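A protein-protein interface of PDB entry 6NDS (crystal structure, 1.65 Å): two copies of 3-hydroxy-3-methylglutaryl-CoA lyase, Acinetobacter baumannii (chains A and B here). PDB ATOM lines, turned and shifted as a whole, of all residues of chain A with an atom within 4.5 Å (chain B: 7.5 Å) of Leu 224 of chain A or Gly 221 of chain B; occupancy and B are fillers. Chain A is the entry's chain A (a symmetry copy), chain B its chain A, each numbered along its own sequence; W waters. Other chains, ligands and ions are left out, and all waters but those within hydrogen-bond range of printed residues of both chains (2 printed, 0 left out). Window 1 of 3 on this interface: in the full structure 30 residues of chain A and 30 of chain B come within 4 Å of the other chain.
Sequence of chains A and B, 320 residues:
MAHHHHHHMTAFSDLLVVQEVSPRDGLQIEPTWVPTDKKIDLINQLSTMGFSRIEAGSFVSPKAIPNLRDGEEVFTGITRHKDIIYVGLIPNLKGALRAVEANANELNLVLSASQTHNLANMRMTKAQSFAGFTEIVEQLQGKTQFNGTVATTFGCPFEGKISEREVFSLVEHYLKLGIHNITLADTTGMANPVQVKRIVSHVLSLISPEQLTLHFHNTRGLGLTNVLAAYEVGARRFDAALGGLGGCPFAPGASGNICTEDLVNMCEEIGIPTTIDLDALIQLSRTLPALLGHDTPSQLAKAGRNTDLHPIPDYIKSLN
Leu 222 of chain A touches Leu 224 of chain B, and with the chains exchanged Leu 224 of chain A touches Leu 222 of chain B.
Leu 224 of chain A touches Thr 225 of chain B, and with the chains exchanged Thr 225 of chain A touches Leu 224 of chain B.
Thr 225 of chain A touches its own counterpart, Thr 225 of chain B.
Positions printed for both chains: 222, 223, 224, 225 and 226.
Of the 12 pairs that touch across the chains among the printed residues, 5 have their exchanged pair printed and touching as well.
CD2 of Leu 222 of chain A touches CD1 of Leu 224 of chain B (3.9 Å).
CD1 of Leu 224 of chain A touches O of Gly 221 of chain B, 3.6 Å away.
CD2 of Leu 222 of chain B touches CD1 of Leu 224 of chain A, 3.9 Å away.
C of Leu 224 of chain A touches OG1 of Thr 225 of chain B (3.9 Å).
OG1 of Thr 225 of chain A touches C of Leu 224 of chain B, at 3.9 Å.
Thr 225 of chain B touches Leu 228 of chain A (CG2 to CD2, 3.6 Å).
Met 266 of chain A touches Leu 222 of chain B (CG to CD2, 3.7 Å).
Thr 219 of chain B touches Gln 299 of chain A (O to CB, 3.4 Å).
Gln 299 of chain A touches Arg 220 of chain B.
CG of Gln 299 of chain A touches N of Gly 221 of chain B, 3.8 Å away.
The backbone carbonyl oxygen (O) of Gly 189 of chain B sits at hydrogen-bond distance from the guanidinium group (NH1) of Arg 220 of chain B (3.3 Å).
The side-chain carboxylate (OD2) of Asp 262 of chain A lies within hydrogen-bond range of the backbone NH (N) of Gln 299 of chain A, at 3.0 Å.
O of Leu 222 of chain B lies close to ND2 of Asn 226 of chain B (3.3 Å).
OD1 of Asn 218 of chain B lies within hydrogen-bond range of N of Leu 222 of chain B, at 3.4 Å.
The side-chain amide nitrogen of Asn 226 of chain A sits close to the backbone carbonyl oxygen of Leu 222 of chain A, at 3.3 Å.
The side-chain hydroxyl (OG) of Ser 255 of chain B lies within hydrogen-bond range of the side-chain hydroxyl (OG1) of Thr 219 of chain B (3.1 Å).
Printed residues of chain B that touch a printed residue of chain A: Asn 218, Thr 219, Arg 220, Gly 221, Leu 222, Leu 224 and Thr 225.
Of the 12 printed residues of chain A, 6 touch a printed residue of chain B.
Hydrophobic or aromatic side chains of chain A within 4 Å of the printed part of chain B: Leu 222, Leu 224, Leu 228 and Met 266.
Of the printed residues of chain B, Leu 224 of chain A touches Gly 221, Leu 222 and Thr 225.
No residue of chain B comes within 4 Å of Gly 223 of chain A.
Of the printed residues of chain A, Thr 225 of chain B touches Leu 224, Thr 225 and Leu 228.
Printed residues of chain B within 4 Å of Leu 228 of chain A: Thr 225 (3.6 Å).
Of the printed residues of chain B, Met 266 of chain A touches Leu 222.
The nearest printed residue of chain B that does not touch Leu 222 of chain A is Thr 225 of chain B (6.2 Å).
OG1 of Thr 225 of chain B lies within hydrogen-bond range of OG1 of Thr 225 of chain A, at 2.9 Å.
The backbone carbonyl oxygen (O) of Asn 218 of chain B lies close to the side-chain amide oxygen (OE1) of Gln 299 of chain A (2.9 Å).
Water W2 bridges O of Thr 219 of chain B (2.7 Å) and O of Gln 299 of chain A (3.0 Å).
Water W1 lies within hydrogen-bond range of O of Arg 220 of chain B, O of Asp 262 of chain A and N of Met 266 of chain A.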
ATOM      1  N   LEU A 222      -6.145 -10.056  17.575  1.00  0.00           N
ATOM      2  CA  LEU A 222      -6.001 -10.463  16.182  1.00  0.00           C
ATOM      3  C   LEU A 222      -5.953  -9.294  15.210  1.00  0.00           C
ATOM      4  O   LEU A 222      -5.942  -9.517  13.989  1.00  0.00           O
ATOM      5  CB  LEU A 222      -7.142 -11.407  15.791  1.00  0.00           C
ATOM      6  CG  LEU A 222      -7.137 -12.702  16.594  1.00  0.00           C
ATOM      7  CD1 LEU A 222      -8.293 -13.570  16.150  1.00  0.00           C
ATOM      8  CD2 LEU A 222      -5.809 -13.419  16.439  1.00  0.00           C
ATOM      9  N   GLY A 223      -5.891  -8.058  15.707  1.00  0.00           N
ATOM     10  CA  GLY A 223      -5.957  -6.909  14.833  1.00  0.00           C
ATOM     11  C   GLY A 223      -4.953  -6.894  13.695  1.00  0.00           C
ATOM     12  O   GLY A 223      -5.345  -6.762  12.529  1.00  0.00           O
ATOM     13  N   LEU A 224      -3.657  -7.013  13.998  1.00  0.00           N
ATOM     14  CA  LEU A 224      -2.670  -6.947  12.918  1.00  0.00           C
ATOM     15  C   LEU A 224      -2.709  -8.196  12.046  1.00  0.00           C
ATOM     16  O   LEU A 224      -2.426  -8.114  10.845  1.00  0.00           O
ATOM     17  CB  LEU A 224      -1.260  -6.734  13.483  1.00  0.00           C
ATOM     18  CG  LEU A 224      -1.051  -5.365  14.143  1.00  0.00           C
ATOM     19  CD1 LEU A 224       0.379  -5.287  14.641  1.00  0.00           C
ATOM     20  CD2 LEU A 224      -1.344  -4.246  13.146  1.00  0.00           C
ATOM     21  N   THR A 225      -3.054  -9.349  12.623  1.00  0.00           N
ATOM     22  CA  THR A 225      -3.205 -10.559  11.817  1.00  0.00           C
ATOM     23  C   THR A 225      -4.346 -10.396  10.817  1.00  0.00           C
ATOM     24  O   THR A 225      -4.241 -10.820   9.656  1.00  0.00           O
ATOM     25  CB  THR A 225      -3.428 -11.763  12.729  1.00  0.00           C
ATOM     26  OG1 THR A 225      -2.371 -11.799  13.705  1.00  0.00           O
ATOM     27  CG2 THR A 225      -3.404 -13.039  11.938  1.00  0.00           C
ATOM     28  N   ASN A 226      -5.419  -9.730  11.238  1.00  0.00           N
ATOM     29  CA  ASN A 226      -6.534  -9.473  10.330  1.00  0.00           C
ATOM     30  C   ASN A 226      -6.166  -8.454   9.256  1.00  0.00           C
ATOM     31  O   ASN A 226      -6.645  -8.556   8.117  1.00  0.00           O
ATOM     32  CB  ASN A 226      -7.757  -8.999  11.125  1.00  0.00           C
ATOM     33  CG  ASN A 226      -8.384 -10.096  11.947  1.00  0.00           C
ATOM     34  OD1 ASN A 226      -8.312 -11.285  11.601  1.00  0.00           O
ATOM     35  ND2 ASN A 226      -9.056  -9.711  13.054  1.00  0.00           N
ATOM     36  N   VAL A 227      -5.375  -7.429   9.602  1.00  0.00           N
ATOM     37  CA  VAL A 227      -4.882  -6.495   8.586  1.00  0.00           C
ATOM     38  C   VAL A 227      -4.117  -7.245   7.509  1.00  0.00           C
ATOM     39  O   VAL A 227      -4.346  -7.046   6.311  1.00  0.00           O
ATOM     40  CB  VAL A 227      -3.989  -5.408   9.214  1.00  0.00           C
ATOM     41  CG1 VAL A 227      -3.264  -4.614   8.102  1.00  0.00           C
ATOM     42  CG2 VAL A 227      -4.833  -4.489  10.061  1.00  0.00           C
ATOM     43  N   LEU A 228      -3.154  -8.072   7.918  1.00  0.00           N
ATOM     44  CA  LEU A 228      -2.324  -8.757   6.929  1.00  0.00           C
ATOM     45  C   LEU A 228      -3.156  -9.722   6.091  1.00  0.00           C
ATOM     46  O   LEU A 228      -2.938  -9.849   4.878  1.00  0.00           O
ATOM     47  CB  LEU A 228      -1.163  -9.475   7.633  1.00  0.00           C
ATOM     48  CG  LEU A 228       0.019  -9.882   6.746  1.00  0.00           C
ATOM     49  CD1 LEU A 228       0.570  -8.679   6.001  1.00  0.00           C
ATOM     50  CD2 LEU A 228       1.112 -10.541   7.591  1.00  0.00           C
ATOM     51  N   ILE A 258      -6.648  -0.932  16.355  1.00  0.00           N
ATOM     52  CA  ILE A 258      -5.259  -1.306  16.121  1.00  0.00           C
ATOM     53  C   ILE A 258      -4.381  -0.068  16.249  1.00  0.00           C
ATOM     54  O   ILE A 258      -4.765   1.055  15.885  1.00  0.00           O
ATOM     55  CB  ILE A 258      -5.058  -1.999  14.766  1.00  0.00           C
ATOM     56  CG1 ILE A 258      -5.561  -1.137  13.623  1.00  0.00           C
ATOM     57  CG2 ILE A 258      -5.736  -3.378  14.761  1.00  0.00           C
ATOM     58  CD1 ILE A 258      -5.050  -1.618  12.255  1.00  0.00           C
ATOM     59  N   ASP A 262       2.191   0.500  15.654  1.00  0.00           N
ATOM     60  CA  ASP A 262       2.425  -0.935  15.510  1.00  0.00           C
ATOM     61  C   ASP A 262       2.096  -1.402  14.090  1.00  0.00           C
ATOM     62  O   ASP A 262       2.812  -2.239  13.531  1.00  0.00           O
ATOM     63  CB  ASP A 262       1.612  -1.726  16.548  1.00  0.00           C
ATOM     64  CG  ASP A 262       2.034  -1.438  17.999  1.00  0.00           C
ATOM     65  OD1 ASP A 262       2.981  -0.652  18.218  1.00  0.00           O
ATOM     66  OD2 ASP A 262       1.409  -2.002  18.934  1.00  0.00           O
ATOM     67  N   LEU A 263       1.025  -0.867  13.488  1.00  0.00           N
ATOM     68  CA  LEU A 263       0.709  -1.186  12.091  1.00  0.00           C
ATOM     69  C   LEU A 263       1.804  -0.707  11.144  1.00  0.00           C
ATOM     70  O   LEU A 263       2.259  -1.455  10.265  1.00  0.00           O
ATOM     71  CB  LEU A 263      -0.635  -0.557  11.711  1.00  0.00           C
ATOM     72  CG  LEU A 263      -0.969  -0.533  10.215  1.00  0.00           C
ATOM     73  CD1 LEU A 263      -1.094  -1.951   9.679  1.00  0.00           C
ATOM     74  CD2 LEU A 263      -2.271   0.258   9.984  1.00  0.00           C
ATOM     75  N   MET A 266       4.865  -2.860  11.412  1.00  0.00           N
ATOM     76  CA  MET A 266       4.679  -4.121  10.702  1.00  0.00           C
ATOM     77  C   MET A 266       4.946  -3.955   9.207  1.00  0.00           C
ATOM     78  O   MET A 266       5.675  -4.752   8.595  1.00  0.00           O
ATOM     79  CB  MET A 266       3.256  -4.638  10.928  1.00  0.00           C
ATOM     80  CG  MET A 266       3.013  -5.942  10.162  1.00  0.00           C
ATOM     81  SD  MET A 266       1.423  -6.735  10.487  1.00  0.00           S
ATOM     82  CE  MET A 266       0.302  -5.719   9.525  1.00  0.00           C
ATOM     83  N   GLN A 299       2.669  -1.312  21.560  1.00  0.00           N
ATOM     84  CA  GLN A 299       3.884  -2.088  21.786  1.00  0.00           C
ATOM     85  C   GLN A 299       5.120  -1.301  21.369  1.00  0.00           C
ATOM     86  O   GLN A 299       6.150  -1.353  22.054  1.00  0.00           O
ATOM     87  CB  GLN A 299       3.815  -3.424  21.044  1.00  0.00           C
ATOM     88  CG  GLN A 299       2.717  -4.362  21.535  1.00  0.00           C
ATOM     89  CD  GLN A 299       2.935  -4.817  22.965  1.00  0.00           C
ATOM     90  OE1 GLN A 299       3.615  -5.814  23.219  1.00  0.00           O
ATOM     91  NE2 GLN A 299       2.358  -4.090  23.907  1.00  0.00           N
ATOM     92  N   GLY B 189      11.352 -10.248  20.377  1.00  0.00           N
ATOM     93  CA  GLY B 189      10.234  -9.876  19.530  1.00  0.00           C
ATOM     94  C   GLY B 189      10.633  -9.008  18.355  1.00  0.00           C
ATOM     95  O   GLY B 189      10.006  -7.977  18.086  1.00  0.00           O
ATOM     96  N   ALA B 191      11.081 -10.424  15.161  1.00  0.00           N
ATOM     97  CA  ALA B 191      10.752 -11.111  13.912  1.00  0.00           C
ATOM     98  C   ALA B 191       9.569 -10.465  13.184  1.00  0.00           C
ATOM     99  O   ALA B 191       8.695  -9.843  13.794  1.00  0.00           O
ATOM    100  CB  ALA B 191      10.423 -12.583  14.177  1.00  0.00           C
ATOM    101  N   HIS B 217       8.231 -13.993  21.097  1.00  0.00           N
ATOM    102  CA  HIS B 217       7.782 -12.990  22.051  1.00  0.00           C
ATOM    103  C   HIS B 217       7.026 -11.894  21.293  1.00  0.00           C
ATOM    104  O   HIS B 217       7.176 -11.733  20.075  1.00  0.00           O
ATOM    105  CB  HIS B 217       8.972 -12.433  22.851  1.00  0.00           C
ATOM    106  CG  HIS B 217       9.532 -13.400  23.864  1.00  0.00           C
ATOM    107  ND1 HIS B 217       9.275 -13.289  25.218  1.00  0.00           N
ATOM    108  CD2 HIS B 217      10.329 -14.486  23.726  1.00  0.00           C
ATOM    109  CE1 HIS B 217       9.889 -14.263  25.865  1.00  0.00           C
ATOM    110  NE2 HIS B 217      10.525 -15.013  24.981  1.00  0.00           N
ATOM    111  N   ASN B 218       6.162 -11.170  22.014  1.00  0.00           N
ATOM    112  CA  ASN B 218       5.218 -10.237  21.399  1.00  0.00           C
ATOM    113  C   ASN B 218       5.642  -8.773  21.555  1.00  0.00           C
ATOM    114  O   ASN B 218       4.794  -7.865  21.533  1.00  0.00           O
ATOM    115  CB  ASN B 218       3.819 -10.443  21.981  1.00  0.00           C
ATOM    116  CG  ASN B 218       2.739  -9.766  21.147  1.00  0.00           C
ATOM    117  OD1 ASN B 218       2.770  -9.813  19.913  1.00  0.00           O
ATOM    118  ND2 ASN B 218       1.788  -9.122  21.816  1.00  0.00           N
ATOM    119  N   THR B 219       6.953  -8.528  21.647  1.00  0.00           N
ATOM    120  CA  THR B 219       7.476  -7.221  22.040  1.00  0.00           C
ATOM    121  C   THR B 219       7.015  -6.111  21.112  1.00  0.00           C
ATOM    122  O   THR B 219       6.811  -4.978  21.566  1.00  0.00           O
ATOM    123  CB  THR B 219       9.002  -7.294  22.073  1.00  0.00           C
ATOM    124  OG1 THR B 219       9.374  -8.477  22.786  1.00  0.00           O
ATOM    125  CG2 THR B 219       9.606  -6.064  22.744  1.00  0.00           C
ATOM    126  N   ARG B 220       6.869  -6.401  19.816  1.00  0.00           N
ATOM    127  CA  ARG B 220       6.410  -5.386  18.877  1.00  0.00           C
ATOM    128  C   ARG B 220       5.060  -5.742  18.271  1.00  0.00           C
ATOM    129  O   ARG B 220       4.681  -5.201  17.226  1.00  0.00           O
ATOM    130  CB  ARG B 220       7.485  -5.128  17.819  1.00  0.00           C
ATOM    131  CG  ARG B 220       8.625  -4.327  18.487  1.00  0.00           C
ATOM    132  CD  ARG B 220       9.941  -4.373  17.790  1.00  0.00           C
ATOM    133  NE  ARG B 220      10.965  -3.715  18.606  1.00  0.00           N
ATOM    134  CZ  ARG B 220      11.864  -4.351  19.353  1.00  0.00           C
ATOM    135  NH1 ARG B 220      11.895  -5.676  19.390  1.00  0.00           N
ATOM    136  NH2 ARG B 220      12.751  -3.654  20.044  1.00  0.00           N
ATOM    137  N   GLY B 221       4.296  -6.584  18.959  1.00  0.00           N
ATOM    138  CA  GLY B 221       2.915  -6.822  18.579  1.00  0.00           C
ATOM    139  C   GLY B 221       2.720  -7.748  17.407  1.00  0.00           C
ATOM    140  O   GLY B 221       1.589  -7.847  16.903  1.00  0.00           O
ATOM    141  N   LEU B 222       3.773  -8.424  16.945  1.00  0.00           N
ATOM    142  CA  LEU B 222       3.678  -9.303  15.784  1.00  0.00           C
ATOM    143  C   LEU B 222       3.642 -10.780  16.144  1.00  0.00           C
ATOM    144  O   LEU B 222       3.672 -11.628  15.238  1.00  0.00           O
ATOM    145  CB  LEU B 222       4.845  -9.036  14.829  1.00  0.00           C
ATOM    146  CG  LEU B 222       4.836  -7.621  14.266  1.00  0.00           C
ATOM    147  CD1 LEU B 222       6.018  -7.443  13.340  1.00  0.00           C
ATOM    148  CD2 LEU B 222       3.524  -7.338  13.557  1.00  0.00           C
ATOM    149  N   GLY B 223       3.546 -11.118  17.430  1.00  0.00           N
ATOM    150  CA  GLY B 223       3.621 -12.504  17.835  1.00  0.00           C
ATOM    151  C   GLY B 223       2.652 -13.442  17.139  1.00  0.00           C
ATOM    152  O   GLY B 223       3.077 -14.451  16.564  1.00  0.00           O
ATOM    153  N   LEU B 224       1.349 -13.148  17.184  1.00  0.00           N
ATOM    154  CA  LEU B 224       0.395 -14.070  16.563  1.00  0.00           C
ATOM    155  C   LEU B 224       0.480 -14.025  15.043  1.00  0.00           C
ATOM    156  O   LEU B 224       0.233 -15.043  14.385  1.00  0.00           O
ATOM    157  CB  LEU B 224      -1.035 -13.765  17.028  1.00  0.00           C
ATOM    158  CG  LEU B 224      -1.285 -14.053  18.514  1.00  0.00           C
ATOM    159  CD1 LEU B 224      -2.731 -13.722  18.828  1.00  0.00           C
ATOM    160  CD2 LEU B 224      -0.979 -15.515  18.828  1.00  0.00           C
ATOM    161  N   THR B 225       0.825 -12.870  14.471  1.00  0.00           N
ATOM    162  CA  THR B 225       1.019 -12.794  13.025  1.00  0.00           C
ATOM    163  C   THR B 225       2.188 -13.677  12.595  1.00  0.00           C
ATOM    164  O   THR B 225       2.125 -14.359  11.561  1.00  0.00           O
ATOM    165  CB  THR B 225       1.233 -11.341  12.607  1.00  0.00           C
ATOM    166  OG1 THR B 225       0.148 -10.552  13.126  1.00  0.00           O
ATOM    167  CG2 THR B 225       1.253 -11.217  11.110  1.00  0.00           C
ATOM    168  N   ASN B 226       3.237 -13.719  13.414  1.00  0.00           N
ATOM    169  CA  ASN B 226       4.375 -14.584  13.114  1.00  0.00           C
ATOM    170  C   ASN B 226       4.025 -16.059  13.282  1.00  0.00           C
ATOM    171  O   ASN B 226       4.540 -16.906  12.537  1.00  0.00           O
ATOM    172  CB  ASN B 226       5.565 -14.209  14.006  1.00  0.00           C
ATOM    173  CG  ASN B 226       6.184 -12.886  13.633  1.00  0.00           C
ATOM    174  OD1 ASN B 226       6.141 -12.457  12.470  1.00  0.00           O
ATOM    175  ND2 ASN B 226       6.816 -12.215  14.621  1.00  0.00           N
ATOM    176  N   SER B 255      10.055  -8.728  26.810  1.00  0.00           N
ATOM    177  CA  SER B 255       8.678  -8.657  27.278  1.00  0.00           C
ATOM    178  C   SER B 255       8.026 -10.015  27.034  1.00  0.00           C
ATOM    179  O   SER B 255       8.697 -11.009  26.736  1.00  0.00           O
ATOM    180  CB  SER B 255       7.938  -7.496  26.596  1.00  0.00           C
ATOM    181  OG  SER B 255       7.662  -7.806  25.243  1.00  0.00           O
HETATM  182  O   HOH W   1       4.713  -4.084  14.636  1.00  0.00           O
HETATM  183  O   HOH W   2       6.465  -3.723  23.920  1.00  0.00           O
